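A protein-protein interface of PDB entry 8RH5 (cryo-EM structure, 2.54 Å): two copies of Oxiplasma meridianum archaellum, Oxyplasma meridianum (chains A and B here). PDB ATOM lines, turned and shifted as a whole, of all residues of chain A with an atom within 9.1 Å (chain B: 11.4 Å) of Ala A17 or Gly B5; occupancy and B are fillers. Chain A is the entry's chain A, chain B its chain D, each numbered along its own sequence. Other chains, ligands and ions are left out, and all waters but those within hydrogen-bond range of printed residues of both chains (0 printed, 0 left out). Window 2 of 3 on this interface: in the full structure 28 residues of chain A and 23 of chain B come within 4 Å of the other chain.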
ATOM      1  N   PHE A  10     -12.050  -0.337 -25.388  1.00  0.00           N
ATOM      2  CA  PHE A  10     -12.651  -1.306 -24.480  1.00  0.00           C
ATOM      3  C   PHE A  10     -11.927  -1.314 -23.132  1.00  0.00           C
ATOM      4  O   PHE A  10     -12.578  -1.356 -22.090  1.00  0.00           O
ATOM      5  CB  PHE A  10     -12.709  -2.693 -25.131  1.00  0.00           C
ATOM      6  CG  PHE A  10     -12.985  -3.845 -24.195  1.00  0.00           C
ATOM      7  CD1 PHE A  10     -14.267  -4.085 -23.715  1.00  0.00           C
ATOM      8  CD2 PHE A  10     -11.964  -4.697 -23.796  1.00  0.00           C
ATOM      9  CE1 PHE A  10     -14.518  -5.145 -22.853  1.00  0.00           C
ATOM     10  CE2 PHE A  10     -12.213  -5.758 -22.935  1.00  0.00           C
ATOM     11  CZ  PHE A  10     -13.491  -5.979 -22.466  1.00  0.00           C
ATOM     12  N   ILE A  11     -10.586  -1.274 -23.175  1.00  0.00           N
ATOM     13  CA  ILE A  11      -9.732  -1.278 -21.995  1.00  0.00           C
ATOM     14  C   ILE A  11     -10.001  -0.018 -21.168  1.00  0.00           C
ATOM     15  O   ILE A  11     -10.087  -0.091 -19.941  1.00  0.00           O
ATOM     16  CB  ILE A  11      -8.242  -1.437 -22.382  1.00  0.00           C
ATOM     17  CG1 ILE A  11      -7.982  -2.758 -23.114  1.00  0.00           C
ATOM     18  CG2 ILE A  11      -7.332  -1.286 -21.168  1.00  0.00           C
ATOM     19  CD1 ILE A  11      -6.760  -2.754 -24.010  1.00  0.00           C
ATOM     20  N   ALA A  12     -10.161   1.119 -21.860  1.00  0.00           N
ATOM     21  CA  ALA A  12     -10.385   2.421 -21.247  1.00  0.00           C
ATOM     22  C   ALA A  12     -11.754   2.481 -20.570  1.00  0.00           C
ATOM     23  O   ALA A  12     -11.889   3.114 -19.523  1.00  0.00           O
ATOM     24  CB  ALA A  12     -10.231   3.508 -22.281  1.00  0.00           C
ATOM     25  N   MET A  13     -12.751   1.818 -21.175  1.00  0.00           N
ATOM     26  CA  MET A  13     -14.126   1.803 -20.696  1.00  0.00           C
ATOM     27  C   MET A  13     -14.228   1.049 -19.371  1.00  0.00           C
ATOM     28  O   MET A  13     -15.012   1.431 -18.503  1.00  0.00           O
ATOM     29  CB  MET A  13     -15.057   1.140 -21.718  1.00  0.00           C
ATOM     30  CG  MET A  13     -15.438   2.037 -22.882  1.00  0.00           C
ATOM     31  SD  MET A  13     -16.735   3.229 -22.467  1.00  0.00           S
ATOM     32  CE  MET A  13     -17.173   3.806 -24.105  1.00  0.00           C
ATOM     33  N   VAL A  14     -13.431  -0.020 -19.241  1.00  0.00           N
ATOM     34  CA  VAL A  14     -13.419  -0.893 -18.074  1.00  0.00           C
ATOM     35  C   VAL A  14     -12.803  -0.146 -16.889  1.00  0.00           C
ATOM     36  O   VAL A  14     -13.305  -0.247 -15.769  1.00  0.00           O
ATOM     37  CB  VAL A  14     -12.703  -2.227 -18.384  1.00  0.00           C
ATOM     38  CG1 VAL A  14     -12.396  -3.045 -17.138  1.00  0.00           C
ATOM     39  CG2 VAL A  14     -13.483  -3.073 -19.380  1.00  0.00           C
ATOM     40  N   LEU A  15     -11.736   0.620 -17.161  1.00  0.00           N
ATOM     41  CA  LEU A  15     -10.976   1.337 -16.148  1.00  0.00           C
ATOM     42  C   LEU A  15     -11.785   2.500 -15.576  1.00  0.00           C
ATOM     43  O   LEU A  15     -11.664   2.805 -14.391  1.00  0.00           O
ATOM     44  CB  LEU A  15      -9.653   1.823 -16.753  1.00  0.00           C
ATOM     45  CG  LEU A  15      -8.564   0.764 -16.935  1.00  0.00           C
ATOM     46  CD1 LEU A  15      -7.565   1.190 -18.000  1.00  0.00           C
ATOM     47  CD2 LEU A  15      -7.848   0.471 -15.623  1.00  0.00           C
ATOM     48  N   VAL A  16     -12.606   3.136 -16.428  1.00  0.00           N
ATOM     49  CA  VAL A  16     -13.424   4.283 -16.059  1.00  0.00           C
ATOM     50  C   VAL A  16     -14.560   3.832 -15.138  1.00  0.00           C
ATOM     51  O   VAL A  16     -14.878   4.520 -14.167  1.00  0.00           O
ATOM     52  CB  VAL A  16     -13.923   5.049 -17.305  1.00  0.00           C
ATOM     53  CG1 VAL A  16     -15.129   5.939 -17.026  1.00  0.00           C
ATOM     54  CG2 VAL A  16     -12.813   5.863 -17.951  1.00  0.00           C
ATOM     55  N   ALA A  17     -15.139   2.661 -15.441  1.00  0.00           N
ATOM     56  CA  ALA A  17     -16.264   2.099 -14.704  1.00  0.00           C
ATOM     57  C   ALA A  17     -15.844   1.663 -13.301  1.00  0.00           C
ATOM     58  O   ALA A  17     -16.670   1.644 -12.389  1.00  0.00           O
ATOM     59  CB  ALA A  17     -16.870   0.958 -15.483  1.00  0.00           C
ATOM     60  N   ALA A  18     -14.557   1.320 -13.146  1.00  0.00           N
ATOM     61  CA  ALA A  18     -13.979   0.900 -11.878  1.00  0.00           C
ATOM     62  C   ALA A  18     -13.841   2.089 -10.926  1.00  0.00           C
ATOM     63  O   ALA A  18     -13.961   1.920  -9.713  1.00  0.00           O
ATOM     64  CB  ALA A  18     -12.650   0.229 -12.118  1.00  0.00           C
ATOM     65  N   VAL A  19     -13.588   3.277 -11.495  1.00  0.00           N
ATOM     66  CA  VAL A  19     -13.365   4.511 -10.753  1.00  0.00           C
ATOM     67  C   VAL A  19     -14.659   4.925 -10.048  1.00  0.00           C
ATOM     68  O   VAL A  19     -14.639   5.221  -8.854  1.00  0.00           O
ATOM     69  CB  VAL A  19     -12.798   5.628 -11.657  1.00  0.00           C
ATOM     70  CG1 VAL A  19     -12.824   7.001 -10.997  1.00  0.00           C
ATOM     71  CG2 VAL A  19     -11.391   5.309 -12.145  1.00  0.00           C
ATOM     72  N   ALA A  20     -15.771   4.916 -10.797  1.00  0.00           N
ATOM     73  CA  ALA A  20     -17.080   5.330 -10.311  1.00  0.00           C
ATOM     74  C   ALA A  20     -17.606   4.356  -9.257  1.00  0.00           C
ATOM     75  O   ALA A  20     -18.369   4.751  -8.377  1.00  0.00           O
ATOM     76  CB  ALA A  20     -18.039   5.459 -11.468  1.00  0.00           C
ATOM     77  N   ALA A  21     -17.189   3.087  -9.369  1.00  0.00           N
ATOM     78  CA  ALA A  21     -17.539   2.031  -8.432  1.00  0.00           C
ATOM     79  C   ALA A  21     -16.866   2.277  -7.082  1.00  0.00           C
ATOM     80  O   ALA A  21     -17.475   2.044  -6.038  1.00  0.00           O
ATOM     81  CB  ALA A  21     -17.150   0.691  -9.008  1.00  0.00           C
ATOM     82  N   THR A  22     -15.617   2.763  -7.126  1.00  0.00           N
ATOM     83  CA  THR A  22     -14.778   2.986  -5.956  1.00  0.00           C
ATOM     84  C   THR A  22     -15.330   4.136  -5.113  1.00  0.00           C
ATOM     85  O   THR A  22     -15.267   4.082  -3.885  1.00  0.00           O
ATOM     86  CB  THR A  22     -13.309   3.185  -6.365  1.00  0.00           C
ATOM     87  OG1 THR A  22     -12.942   2.133  -7.258  1.00  0.00           O
ATOM     88  CG2 THR A  22     -12.350   3.192  -5.194  1.00  0.00           C
ATOM     89  N   VAL A  23     -15.873   5.160  -5.787  1.00  0.00           N
ATOM     90  CA  VAL A  23     -16.405   6.361  -5.156  1.00  0.00           C
ATOM     91  C   VAL A  23     -17.599   5.991  -4.272  1.00  0.00           C
ATOM     92  O   VAL A  23     -17.686   6.451  -3.133  1.00  0.00           O
ATOM     93  CB  VAL A  23     -16.763   7.450  -6.192  1.00  0.00           C
ATOM     94  CG1 VAL A  23     -17.403   8.679  -5.556  1.00  0.00           C
ATOM     95  CG2 VAL A  23     -15.561   7.865  -7.028  1.00  0.00           C
ATOM     96  N   LEU A  24     -18.490   5.142  -4.803  1.00  0.00           N
ATOM     97  CA  LEU A  24     -19.747   4.783  -4.161  1.00  0.00           C
ATOM     98  C   LEU A  24     -19.505   3.929  -2.917  1.00  0.00           C
ATOM     99  O   LEU A  24     -20.237   4.056  -1.937  1.00  0.00           O
ATOM    100  CB  LEU A  24     -20.646   4.056  -5.169  1.00  0.00           C
ATOM    101  CG  LEU A  24     -21.303   4.928  -6.241  1.00  0.00           C
ATOM    102  CD1 LEU A  24     -21.636   4.106  -7.477  1.00  0.00           C
ATOM    103  CD2 LEU A  24     -22.554   5.614  -5.708  1.00  0.00           C
ATOM    104  N   ILE A  25     -18.480   3.066  -2.973  1.00  0.00           N
ATOM    105  CA  ILE A  25     -18.140   2.159  -1.884  1.00  0.00           C
ATOM    106  C   ILE A  25     -17.494   2.946  -0.743  1.00  0.00           C
ATOM    107  O   ILE A  25     -17.842   2.741   0.420  1.00  0.00           O
ATOM    108  CB  ILE A  25     -17.269   0.981  -2.387  1.00  0.00           C
ATOM    109  CG1 ILE A  25     -18.046   0.074  -3.349  1.00  0.00           C
ATOM    110  CG2 ILE A  25     -16.681   0.184  -1.226  1.00  0.00           C
ATOM    111  CD1 ILE A  25     -17.179  -0.788  -4.246  1.00  0.00           C
ATOM    112  N   GLU B   1     -18.079  -1.790 -25.822  1.00  0.00           N
ATOM    113  CA  GLU B   1     -19.530  -1.431 -25.808  1.00  0.00           C
ATOM    114  C   GLU B   1     -19.950  -1.064 -24.384  1.00  0.00           C
ATOM    115  O   GLU B   1     -19.201  -1.283 -23.432  1.00  0.00           O
ATOM    116  CB  GLU B   1     -20.360  -2.568 -26.418  1.00  0.00           C
ATOM    117  CG  GLU B   1     -21.739  -2.152 -26.912  1.00  0.00           C
ATOM    118  CD  GLU B   1     -21.796  -0.961 -27.858  1.00  0.00           C
ATOM    119  OE1 GLU B   1     -22.301   0.099 -27.438  1.00  0.00           O
ATOM    120  OE2 GLU B   1     -21.345  -1.097 -29.013  1.00  0.00           O
ATOM    121  N   THR B   2     -21.164  -0.504 -24.265  1.00  0.00           N
ATOM    122  CA  THR B   2     -21.729  -0.002 -23.022  1.00  0.00           C
ATOM    123  C   THR B   2     -22.106  -1.161 -22.096  1.00  0.00           C
ATOM    124  O   THR B   2     -22.215  -0.973 -20.885  1.00  0.00           O
ATOM    125  CB  THR B   2     -22.908   0.944 -23.303  1.00  0.00           C
ATOM    126  OG1 THR B   2     -22.626   1.716 -24.471  1.00  0.00           O
ATOM    127  CG2 THR B   2     -23.224   1.874 -22.152  1.00  0.00           C
ATOM    128  N   GLY B   3     -22.283  -2.355 -22.681  1.00  0.00           N
ATOM    129  CA  GLY B   3     -22.715  -3.554 -21.976  1.00  0.00           C
ATOM    130  C   GLY B   3     -21.742  -4.002 -20.886  1.00  0.00           C
ATOM    131  O   GLY B   3     -22.172  -4.479 -19.836  1.00  0.00           O
ATOM    132  N   ILE B   4     -20.438  -3.838 -21.152  1.00  0.00           N
ATOM    133  CA  ILE B   4     -19.371  -4.260 -20.255  1.00  0.00           C
ATOM    134  C   ILE B   4     -19.342  -3.342 -19.030  1.00  0.00           C
ATOM    135  O   ILE B   4     -19.276  -3.825 -17.901  1.00  0.00           O
ATOM    136  CB  ILE B   4     -18.007  -4.313 -20.987  1.00  0.00           C
ATOM    137  CG1 ILE B   4     -18.062  -5.080 -22.319  1.00  0.00           C
ATOM    138  CG2 ILE B   4     -16.893  -4.817 -20.075  1.00  0.00           C
ATOM    139  CD1 ILE B   4     -18.426  -6.552 -22.219  1.00  0.00           C
ATOM    140  N   GLY B   5     -19.407  -2.026 -19.278  1.00  0.00           N
ATOM    141  CA  GLY B   5     -19.314  -1.004 -18.247  1.00  0.00           C
ATOM    142  C   GLY B   5     -20.516  -0.993 -17.303  1.00  0.00           C
ATOM    143  O   GLY B   5     -20.379  -0.630 -16.135  1.00  0.00           O
ATOM    144  N   THR B   6     -21.682  -1.393 -17.830  1.00  0.00           N
ATOM    145  CA  THR B   6     -22.939  -1.420 -17.094  1.00  0.00           C
ATOM    146  C   THR B   6     -22.892  -2.496 -16.008  1.00  0.00           C
ATOM    147  O   THR B   6     -23.376  -2.273 -14.900  1.00  0.00           O
ATOM    148  CB  THR B   6     -24.132  -1.560 -18.053  1.00  0.00           C
ATOM    149  OG1 THR B   6     -24.071  -0.498 -19.006  1.00  0.00           O
ATOM    150  CG2 THR B   6     -25.478  -1.527 -17.360  1.00  0.00           C
ATOM    151  N   LEU B   7     -22.286  -3.648 -16.341  1.00  0.00           N
ATOM    152  CA  LEU B   7     -22.239  -4.815 -15.472  1.00  0.00           C
ATOM    153  C   LEU B   7     -21.311  -4.576 -14.282  1.00  0.00           C
ATOM    154  O   LEU B   7     -21.592  -5.053 -13.184  1.00  0.00           O
ATOM    155  CB  LEU B   7     -21.799  -6.038 -16.286  1.00  0.00           C
ATOM    156  CG  LEU B   7     -22.865  -6.678 -17.177  1.00  0.00           C
ATOM    157  CD1 LEU B   7     -22.224  -7.521 -18.269  1.00  0.00           C
ATOM    158  CD2 LEU B   7     -23.840  -7.519 -16.364  1.00  0.00           C
ATOM    159  N   ILE B   8     -20.216  -3.836 -14.515  1.00  0.00           N
ATOM    160  CA  ILE B   8     -19.188  -3.567 -13.516  1.00  0.00           C
ATOM    161  C   ILE B   8     -19.762  -2.672 -12.415  1.00  0.00           C
ATOM    162  O   ILE B   8     -19.557  -2.944 -11.232  1.00  0.00           O
ATOM    163  CB  ILE B   8     -17.911  -2.984 -14.168  1.00  0.00           C
ATOM    164  CG1 ILE B   8     -17.264  -3.978 -15.140  1.00  0.00           C
ATOM    165  CG2 ILE B   8     -16.916  -2.505 -13.115  1.00  0.00           C
ATOM    166  CD1 ILE B   8     -16.365  -3.346 -16.183  1.00  0.00           C
ATOM    167  N   ILE B   9     -20.493  -1.624 -12.822  1.00  0.00           N
ATOM    168  CA  ILE B   9     -21.078  -0.647 -11.911  1.00  0.00           C
ATOM    169  C   ILE B   9     -22.252  -1.281 -11.162  1.00  0.00           C
ATOM    170  O   ILE B   9     -22.503  -0.936 -10.008  1.00  0.00           O
ATOM    171  CB  ILE B   9     -21.447   0.658 -12.657  1.00  0.00           C
ATOM    172  CG1 ILE B   9     -20.206   1.326 -13.262  1.00  0.00           C
ATOM    173  CG2 ILE B   9     -22.213   1.624 -11.759  1.00  0.00           C
ATOM    174  CD1 ILE B   9     -20.495   2.283 -14.399  1.00  0.00           C
ATOM    175  N   PHE B  10     -22.938  -2.231 -11.819  1.00  0.00           N
ATOM    176  CA  PHE B  10     -24.077  -2.950 -11.263  1.00  0.00           C
ATOM    177  C   PHE B  10     -23.682  -3.699  -9.990  1.00  0.00           C
ATOM    178  O   PHE B  10     -24.430  -3.678  -9.012  1.00  0.00           O
ATOM    179  CB  PHE B  10     -24.705  -3.867 -12.319  1.00  0.00           C
ATOM    180  CG  PHE B  10     -25.662  -4.912 -11.796  1.00  0.00           C
ATOM    181  CD1 PHE B  10     -26.954  -4.571 -11.413  1.00  0.00           C
ATOM    182  CD2 PHE B  10     -25.273  -6.241 -11.690  1.00  0.00           C
ATOM    183  CE1 PHE B  10     -27.831  -5.533 -10.931  1.00  0.00           C
ATOM    184  CE2 PHE B  10     -26.150  -7.204 -11.207  1.00  0.00           C
ATOM    185  CZ  PHE B  10     -27.427  -6.848 -10.830  1.00  0.00           C
ATOM    186  N   ILE B  11     -22.509  -4.350 -10.020  1.00  0.00           N
ATOM    187  CA  ILE B  11     -21.974  -5.119  -8.904  1.00  0.00           C
ATOM    188  C   ILE B  11     -21.717  -4.182  -7.720  1.00  0.00           C
ATOM    189  O   ILE B  11     -22.025  -4.530  -6.579  1.00  0.00           O
ATOM    190  CB  ILE B  11     -20.716  -5.916  -9.324  1.00  0.00           C
ATOM    191  CG1 ILE B  11     -21.026  -6.922 -10.438  1.00  0.00           C
ATOM    192  CG2 ILE B  11     -20.060  -6.596  -8.127  1.00  0.00           C
ATOM    193  CD1 ILE B  11     -19.833  -7.310 -11.289  1.00  0.00           C
ATOM    194  N   ALA B  12     -21.179  -2.990  -8.016  1.00  0.00           N
ATOM    195  CA  ALA B  12     -20.829  -1.986  -7.022  1.00  0.00           C
ATOM    196  C   ALA B  12     -22.079  -1.409  -6.358  1.00  0.00           C
ATOM    197  O   ALA B  12     -22.053  -1.111  -5.165  1.00  0.00           O
ATOM    198  CB  ALA B  12     -19.993  -0.904  -7.660  1.00  0.00           C
ATOM    199  N   MET B  13     -23.159  -1.265  -7.139  1.00  0.00           N
ATOM    200  CA  MET B  13     -24.420  -0.692  -6.687  1.00  0.00           C
ATOM    201  C   MET B  13     -25.093  -1.610  -5.668  1.00  0.00           C
ATOM    202  O   MET B  13     -25.716  -1.129  -4.722  1.00  0.00           O
ATOM    203  CB  MET B  13     -25.376  -0.469  -7.864  1.00  0.00           C
ATOM    204  CG  MET B  13     -25.070   0.772  -8.683  1.00  0.00           C
ATOM    205  SD  MET B  13     -25.658   2.298  -7.909  1.00  0.00           S
ATOM    206  CE  MET B  13     -25.481   3.438  -9.279  1.00  0.00           C
ATOM    207  N   LEU B  15     -23.535  -3.852  -3.713  1.00  0.00           N
ATOM    208  CA  LEU B  15     -22.696  -3.941  -2.527  1.00  0.00           C
ATOM    209  C   LEU B  15     -22.908  -2.733  -1.615  1.00  0.00           C
ATOM    210  O   LEU B  15     -22.846  -2.871  -0.394  1.00  0.00           O
ATOM    211  CB  LEU B  15     -21.227  -4.069  -2.950  1.00  0.00           C
ATOM    212  CG  LEU B  15     -20.791  -5.445  -3.460  1.00  0.00           C
ATOM    213  CD1 LEU B  15     -19.554  -5.328  -4.337  1.00  0.00           C
ATOM    214  CD2 LEU B  15     -20.535  -6.409  -2.310  1.00  0.00           C
ATOM    215  N   VAL B  16     -23.157  -1.561  -2.220  1.00  0.00           N
ATOM    216  CA  VAL B  16     -23.350  -0.305  -1.504  1.00  0.00           C
ATOM    217  C   VAL B  16     -24.693  -0.333  -0.771  1.00  0.00           C
ATOM    218  O   VAL B  16     -24.783   0.127   0.368  1.00  0.00           O
ATOM    219  CB  VAL B  16     -23.197   0.912  -2.444  1.00  0.00           C
ATOM    220  CG1 VAL B  16     -23.833   2.183  -1.895  1.00  0.00           C
ATOM    221  CG2 VAL B  16     -21.741   1.170  -2.801  1.00  0.00           C
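Among the printed residues, merely in contact across the chains: Leu A24 with Val B16 (3.4 Å), Ala A21 with Ala B12 (3.5 Å), Phe A10 with Ile B4 (3.6 Å), Ala A17 with Ile B9 (3.7 Å), Ile A25 with Val B16 (3.8 Å), Val A14 with Ile B4 (3.9 Å) and Ala A17 with Gly B5 (3.9 Å).
Printed residues of chain B that touch a printed residue of chain A: Ile B4, Gly B5, Ile B9, Ala B12 and Val B16. Hydrophobic or aromatic side chains of chain B within 4 Å of the printed part of chain A: Ile B4, Ile B9, Ala B12 and Val B16. Along chain B the printed residues that touch a printed residue of chain A span positions 4 to 16. Of the 16 printed residues of chain A, 6 touch a printed residue of chain B. Along chain A the printed residues that touch a printed residue of chain B span positions 10 to 25. Among the printed residues, 7 pairs touch across the chains.
6 positions are printed for both chains.
Ala A17 touches just these residues of chain B: Gly B5 and Ile B9. Of the printed residues of chain A, Gly B5 touches Ala A17 (3.9 Å). Val A14 touches one residue of chain B. No residue of chain B comes within 4 Å of Val A16. Ala A18 touches none of the printed residues of chain B. No residue of chain B comes within 4 Å of Val A19. No residue of chain B comes within 4 Å of Ala A20. Of the printed residues of chain B, Ala A21 touches Ala B12. No residue of chain A comes within 4 Å of Gly B3. Printed residues of chain B within 4 Å of Ile A25: Val B16 (3.8 Å). Printed residues of chain A within 4 Å of Ile B9: Ala A17 (3.7 Å). Printed residues of chain B within 4 Å of Phe A10: Ile B4. Val A23 touches none of the printed residues of chain B. Ile B11 touches none of the printed residues of chain A. The nearest residue of chain A that does not touch Gly B5 is Met A13 (4.9 Å).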
